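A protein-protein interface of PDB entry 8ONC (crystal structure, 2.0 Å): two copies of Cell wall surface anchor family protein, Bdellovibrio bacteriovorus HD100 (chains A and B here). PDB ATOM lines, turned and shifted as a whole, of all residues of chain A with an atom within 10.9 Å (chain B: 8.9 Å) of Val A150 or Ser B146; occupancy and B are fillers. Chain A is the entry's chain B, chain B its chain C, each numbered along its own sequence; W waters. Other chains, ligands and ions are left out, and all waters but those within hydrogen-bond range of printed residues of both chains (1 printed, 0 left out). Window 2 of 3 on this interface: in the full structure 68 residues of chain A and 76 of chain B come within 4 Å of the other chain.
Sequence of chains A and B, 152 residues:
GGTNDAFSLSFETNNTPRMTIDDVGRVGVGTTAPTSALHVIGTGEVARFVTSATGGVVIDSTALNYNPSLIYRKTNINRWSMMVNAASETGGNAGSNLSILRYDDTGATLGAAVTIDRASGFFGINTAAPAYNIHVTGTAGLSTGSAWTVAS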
ATOM      1  N   ILE A 134      -6.859  -0.269   9.112  1.00  0.00           N
ATOM      2  CA  ILE A 134      -6.732  -1.706   8.903  1.00  0.00           C
ATOM      3  C   ILE A 134      -5.496  -1.930   8.043  1.00  0.00           C
ATOM      4  O   ILE A 134      -5.264  -1.200   7.073  1.00  0.00           O
ATOM      5  CB  ILE A 134      -7.991  -2.327   8.264  1.00  0.00           C
ATOM      6  CG1 ILE A 134      -7.863  -3.851   8.216  1.00  0.00           C
ATOM      7  CG2 ILE A 134      -8.266  -1.744   6.883  1.00  0.00           C
ATOM      8  CD1 ILE A 134      -9.119  -4.557   7.748  1.00  0.00           C
ATOM      9  N   ALA A 140      -6.228 -10.482   0.152  1.00  0.00           N
ATOM     10  CA  ALA A 140      -7.534  -9.970   0.553  1.00  0.00           C
ATOM     11  C   ALA A 140      -8.595 -10.440  -0.432  1.00  0.00           C
ATOM     12  O   ALA A 140      -8.464 -10.218  -1.640  1.00  0.00           O
ATOM     13  CB  ALA A 140      -7.526  -8.439   0.628  1.00  0.00           C
ATOM     14  N   LEU A 142     -12.876 -10.576  -1.277  1.00  0.00           N
ATOM     15  CA  LEU A 142     -14.213 -10.040  -1.045  1.00  0.00           C
ATOM     16  C   LEU A 142     -15.180 -10.721  -2.001  1.00  0.00           C
ATOM     17  O   LEU A 142     -14.922 -10.776  -3.208  1.00  0.00           O
ATOM     18  CB  LEU A 142     -14.246  -8.522  -1.251  1.00  0.00           C
ATOM     19  CG  LEU A 142     -15.552  -7.781  -0.952  1.00  0.00           C
ATOM     20  CD1 LEU A 142     -15.904  -7.862   0.527  1.00  0.00           C
ATOM     21  CD2 LEU A 142     -15.457  -6.332  -1.413  1.00  0.00           C
ATOM     22  N   GLY A 145     -17.141  -8.171  -4.912  1.00  0.00           N
ATOM     23  CA  GLY A 145     -16.477  -7.279  -5.839  1.00  0.00           C
ATOM     24  C   GLY A 145     -15.037  -7.050  -5.429  1.00  0.00           C
ATOM     25  O   GLY A 145     -14.524  -7.675  -4.503  1.00  0.00           O
ATOM     26  N   SER A 146     -14.397  -6.127  -6.143  1.00  0.00           N
ATOM     27  CA  SER A 146     -12.985  -5.837  -5.940  1.00  0.00           C
ATOM     28  C   SER A 146     -12.740  -4.527  -5.206  1.00  0.00           C
ATOM     29  O   SER A 146     -11.579  -4.173  -4.976  1.00  0.00           O
ATOM     30  CB  SER A 146     -12.257  -5.802  -7.286  1.00  0.00           C
ATOM     31  OG  SER A 146     -12.773  -4.766  -8.104  1.00  0.00           O
ATOM     32  N   ALA A 147     -13.789  -3.802  -4.829  1.00  0.00           N
ATOM     33  CA  ALA A 147     -13.641  -2.461  -4.285  1.00  0.00           C
ATOM     34  C   ALA A 147     -14.293  -2.343  -2.915  1.00  0.00           C
ATOM     35  O   ALA A 147     -15.291  -3.009  -2.618  1.00  0.00           O
ATOM     36  CB  ALA A 147     -14.251  -1.416  -5.233  1.00  0.00           C
ATOM     37  N   TRP A 148     -13.709  -1.489  -2.077  1.00  0.00           N
ATOM     38  CA  TRP A 148     -14.413  -1.008  -0.899  1.00  0.00           C
ATOM     39  C   TRP A 148     -15.591  -0.143  -1.330  1.00  0.00           C
ATOM     40  O   TRP A 148     -15.531   0.566  -2.337  1.00  0.00           O
ATOM     41  CB  TRP A 148     -13.495  -0.167  -0.008  1.00  0.00           C
ATOM     42  CG  TRP A 148     -12.324  -0.860   0.623  1.00  0.00           C
ATOM     43  CD1 TRP A 148     -11.091  -1.051   0.070  1.00  0.00           C
ATOM     44  CD2 TRP A 148     -12.250  -1.386   1.958  1.00  0.00           C
ATOM     45  NE1 TRP A 148     -10.264  -1.691   0.964  1.00  0.00           N
ATOM     46  CE2 TRP A 148     -10.951  -1.905   2.131  1.00  0.00           C
ATOM     47  CE3 TRP A 148     -13.161  -1.482   3.017  1.00  0.00           C
ATOM     48  CZ2 TRP A 148     -10.537  -2.511   3.320  1.00  0.00           C
ATOM     49  CZ3 TRP A 148     -12.748  -2.085   4.201  1.00  0.00           C
ATOM     50  CH2 TRP A 148     -11.449  -2.593   4.339  1.00  0.00           C
ATOM     51  N   THR A 149     -16.666  -0.196  -0.552  1.00  0.00           N
ATOM     52  CA  THR A 149     -17.743   0.770  -0.701  1.00  0.00           C
ATOM     53  C   THR A 149     -17.406   2.014   0.109  1.00  0.00           C
ATOM     54  O   THR A 149     -17.101   1.920   1.300  1.00  0.00           O
ATOM     55  CB  THR A 149     -19.075   0.177  -0.240  1.00  0.00           C
ATOM     56  OG1 THR A 149     -19.355  -1.013  -0.988  1.00  0.00           O
ATOM     57  CG2 THR A 149     -20.207   1.178  -0.435  1.00  0.00           C
ATOM     58  N   VAL A 150     -17.440   3.177  -0.537  1.00  0.00           N
ATOM     59  CA  VAL A 150     -17.093   4.413   0.158  1.00  0.00           C
ATOM     60  C   VAL A 150     -18.179   4.696   1.192  1.00  0.00           C
ATOM     61  O   VAL A 150     -19.336   4.944   0.841  1.00  0.00           O
ATOM     62  CB  VAL A 150     -16.926   5.586  -0.813  1.00  0.00           C
ATOM     63  CG1 VAL A 150     -16.679   6.871  -0.041  1.00  0.00           C
ATOM     64  CG2 VAL A 150     -15.774   5.313  -1.768  1.00  0.00           C
ATOM     65  N   ALA A 151     -17.809   4.649   2.468  1.00  0.00           N
ATOM     66  CA  ALA A 151     -18.771   4.767   3.555  1.00  0.00           C
ATOM     67  C   ALA A 151     -18.972   6.218   3.978  1.00  0.00           C
ATOM     68  O   ALA A 151     -20.100   6.706   4.045  1.00  0.00           O
ATOM     69  CB  ALA A 151     -18.324   3.928   4.746  1.00  0.00           C
ATOM     70  N   ALA B 140     -17.803  -4.380   2.070  1.00  0.00           N
ATOM     71  CA  ALA B 140     -16.665  -3.801   2.776  1.00  0.00           C
ATOM     72  C   ALA B 140     -16.728  -2.289   2.629  1.00  0.00           C
ATOM     73  O   ALA B 140     -16.677  -1.773   1.509  1.00  0.00           O
ATOM     74  CB  ALA B 140     -15.339  -4.340   2.227  1.00  0.00           C
ATOM     75  N   GLY B 141     -16.839  -1.584   3.752  1.00  0.00           N
ATOM     76  CA  GLY B 141     -16.976  -0.136   3.758  1.00  0.00           C
ATOM     77  C   GLY B 141     -15.702   0.536   4.246  1.00  0.00           C
ATOM     78  O   GLY B 141     -15.120   0.130   5.255  1.00  0.00           O
ATOM     79  N   LEU B 142     -15.284   1.567   3.514  1.00  0.00           N
ATOM     80  CA  LEU B 142     -14.111   2.361   3.852  1.00  0.00           C
ATOM     81  C   LEU B 142     -14.471   3.833   3.718  1.00  0.00           C
ATOM     82  O   LEU B 142     -14.996   4.254   2.682  1.00  0.00           O
ATOM     83  CB  LEU B 142     -12.922   2.015   2.948  1.00  0.00           C
ATOM     84  CG  LEU B 142     -11.565   2.630   3.297  1.00  0.00           C
ATOM     85  CD1 LEU B 142     -11.091   2.145   4.658  1.00  0.00           C
ATOM     86  CD2 LEU B 142     -10.540   2.295   2.222  1.00  0.00           C
ATOM     87  N   SER B 143     -14.183   4.615   4.760  1.00  0.00           N
ATOM     88  CA  SER B 143     -14.631   6.002   4.779  1.00  0.00           C
ATOM     89  C   SER B 143     -13.804   6.908   3.874  1.00  0.00           C
ATOM     90  O   SER B 143     -14.256   8.012   3.551  1.00  0.00           O
ATOM     91  CB  SER B 143     -14.598   6.547   6.206  1.00  0.00           C
ATOM     92  OG  SER B 143     -13.266   6.639   6.681  1.00  0.00           O
ATOM     93  N   THR B 144     -12.618   6.476   3.445  1.00  0.00           N
ATOM     94  CA  THR B 144     -11.682   7.358   2.758  1.00  0.00           C
ATOM     95  C   THR B 144     -11.517   7.057   1.275  1.00  0.00           C
ATOM     96  O   THR B 144     -10.789   7.786   0.593  1.00  0.00           O
ATOM     97  CB  THR B 144     -10.306   7.304   3.436  1.00  0.00           C
ATOM     98  OG1 THR B 144      -9.856   5.946   3.506  1.00  0.00           O
ATOM     99  CG2 THR B 144     -10.382   7.883   4.840  1.00  0.00           C
ATOM    100  N   GLY B 145     -12.153   6.019   0.755  1.00  0.00           N
ATOM    101  CA  GLY B 145     -12.022   5.698  -0.650  1.00  0.00           C
ATOM    102  C   GLY B 145     -12.426   4.262  -0.918  1.00  0.00           C
ATOM    103  O   GLY B 145     -12.906   3.553  -0.035  1.00  0.00           O
ATOM    104  N   SER B 146     -12.205   3.848  -2.167  1.00  0.00           N
ATOM    105  CA  SER B 146     -12.629   2.533  -2.628  1.00  0.00           C
ATOM    106  C   SER B 146     -11.485   1.546  -2.813  1.00  0.00           C
ATOM    107  O   SER B 146     -11.750   0.365  -3.066  1.00  0.00           O
ATOM    108  CB  SER B 146     -13.403   2.654  -3.951  1.00  0.00           C
ATOM    109  OG  SER B 146     -12.549   3.040  -5.014  1.00  0.00           O
ATOM    110  N   ALA B 147     -10.233   1.978  -2.691  1.00  0.00           N
ATOM    111  CA  ALA B 147      -9.095   1.092  -2.890  1.00  0.00           C
ATOM    112  C   ALA B 147      -8.251   0.997  -1.623  1.00  0.00           C
ATOM    113  O   ALA B 147      -8.287   1.874  -0.755  1.00  0.00           O
ATOM    114  CB  ALA B 147      -8.222   1.561  -4.060  1.00  0.00           C
ATOM    115  N   TRP B 148      -7.496  -0.096  -1.524  1.00  0.00           N
ATOM    116  CA  TRP B 148      -6.469  -0.213  -0.500  1.00  0.00           C
ATOM    117  C   TRP B 148      -5.272   0.660  -0.854  1.00  0.00           C
ATOM    118  O   TRP B 148      -4.943   0.853  -2.027  1.00  0.00           O
ATOM    119  CB  TRP B 148      -5.972  -1.656  -0.364  1.00  0.00           C
ATOM    120  CG  TRP B 148      -6.967  -2.699   0.045  1.00  0.00           C
ATOM    121  CD1 TRP B 148      -7.887  -3.311  -0.756  1.00  0.00           C
ATOM    122  CD2 TRP B 148      -7.087  -3.317   1.337  1.00  0.00           C
ATOM    123  NE1 TRP B 148      -8.594  -4.244  -0.037  1.00  0.00           N
ATOM    124  CE2 TRP B 148      -8.123  -4.268   1.249  1.00  0.00           C
ATOM    125  CE3 TRP B 148      -6.434  -3.145   2.563  1.00  0.00           C
ATOM    126  CZ2 TRP B 148      -8.518  -5.046   2.338  1.00  0.00           C
ATOM    127  CZ3 TRP B 148      -6.828  -3.920   3.643  1.00  0.00           C
ATOM    128  CH2 TRP B 148      -7.861  -4.856   3.523  1.00  0.00           C
ATOM    129  N   THR B 149      -4.604   1.170   0.173  1.00  0.00           N
ATOM    130  CA  THR B 149      -3.257   1.692  -0.002  1.00  0.00           C
ATOM    131  C   THR B 149      -2.286   0.520  -0.050  1.00  0.00           C
ATOM    132  O   THR B 149      -2.353  -0.383   0.789  1.00  0.00           O
ATOM    133  CB  THR B 149      -2.883   2.639   1.138  1.00  0.00           C
ATOM    134  OG1 THR B 149      -3.831   3.711   1.211  1.00  0.00           O
ATOM    135  CG2 THR B 149      -1.491   3.212   0.922  1.00  0.00           C
HETATM  136  O   HOH W   1     -18.009  -3.408  -0.796  1.00  0.00           O
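The indole nitrogen (NE1) of Trp A148 sits close to the indole nitrogen (NE1) of Trp B148 (3.2 Å). The backbone NH (N) of Ala A151 sits at hydrogen-bond distance from the backbone carbonyl oxygen (O) of Leu B142 (2.8 Å). The backbone NH (N) of Trp A148 lies within hydrogen-bond range of the backbone carbonyl oxygen (O) of Ser B146 (2.9 Å). N of Thr A149 sits at hydrogen-bond distance from O of Ala B140, at 2.6 Å. The backbone NH of Leu B142 lies within hydrogen-bond range of the backbone carbonyl oxygen of Thr A149 (2.9 Å).
Among the printed residues, pairs that only touch across the chains: Thr A149 with Gly B141, Val A150 with Leu B142, Trp A148 with Gly B141, Trp A148 with Ala B140, Trp A148 with Leu B142, Val A150 with Gly B145, Ala A147 with Ser B146, Trp A148 with Gly B145, Val A150 with Ser B146, Trp A148 with Ala B147, Ala A140 with Trp B148 and Leu A142 with Ala B140.
Printed residues of chain A within 4 Å of Ser B146: Ala A147 (3.6 Å), Trp A148 (2.9 Å) and Val A150 (3.9 Å). Of chain B, only Leu B142 (2.8 Å) comes within 4 Å of Ala A151. Gly B141 touches just these residues of chain A: Trp A148 (3.4 Å) and Thr A149 (3.2 Å). Gly B145 touches just these residues of chain A: Trp A148 (3.8 Å) and Val A150 (3.6 Å). Ala B147 touches just one residue of chain A: Trp A148. Of the printed residues of chain B, Leu A142 touches Ala B140 (3.95 Å). Of the printed residues of chain B, Ala A140 touches Trp B148 (3.9 Å). Printed residues of chain A within 4 Å of Trp B148: Ala A140 and Trp A148. Of the printed residues of chain A, Ala B140 touches Leu A142 (3.95 Å), Trp A148 (3.4 Å) and Thr A149 (2.6 Å). The nearest residue of chain A that does not touch Ser B146 is Ser A146 (4.9 Å). The nearest printed residue of chain B that does not touch Ala A147 is Ala B140 (4.5 Å).
Of the 10 printed residues of chain A, 7 touch a printed residue of chain B. Hydrophobic or aromatic side chains of chain A within 4 Å of the printed part of chain B: Ala A140, Leu A142, Ala A147, Trp A148, Val A150 and Ala A151.
Trp A148 touches Leu B142, but with the chains exchanged Leu A142 does not touch Trp B148 (7.2 Å). Trp A148 touches Gly B145, but with the chains exchanged Gly A145 does not touch Trp B148 (8.2 Å). Trp A148 touches Ser B146, but with the chains exchanged Ser A146 does not touch Trp B148 (5.7 Å). Trp B148 touches its own counterpart, Trp A148. Of the 17 pairs that touch across the chains among the printed residues, 3 have their exchanged pair printed and touching as well.
Water W1 lies within hydrogen-bond range of the side-chain hydroxyl (OG1) of Thr A149 (2.8 Å), the backbone NH (N) of Ala B140 (3.0 Å) and the backbone carbonyl oxygen (O) of Ala A147 (3.3 Å).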
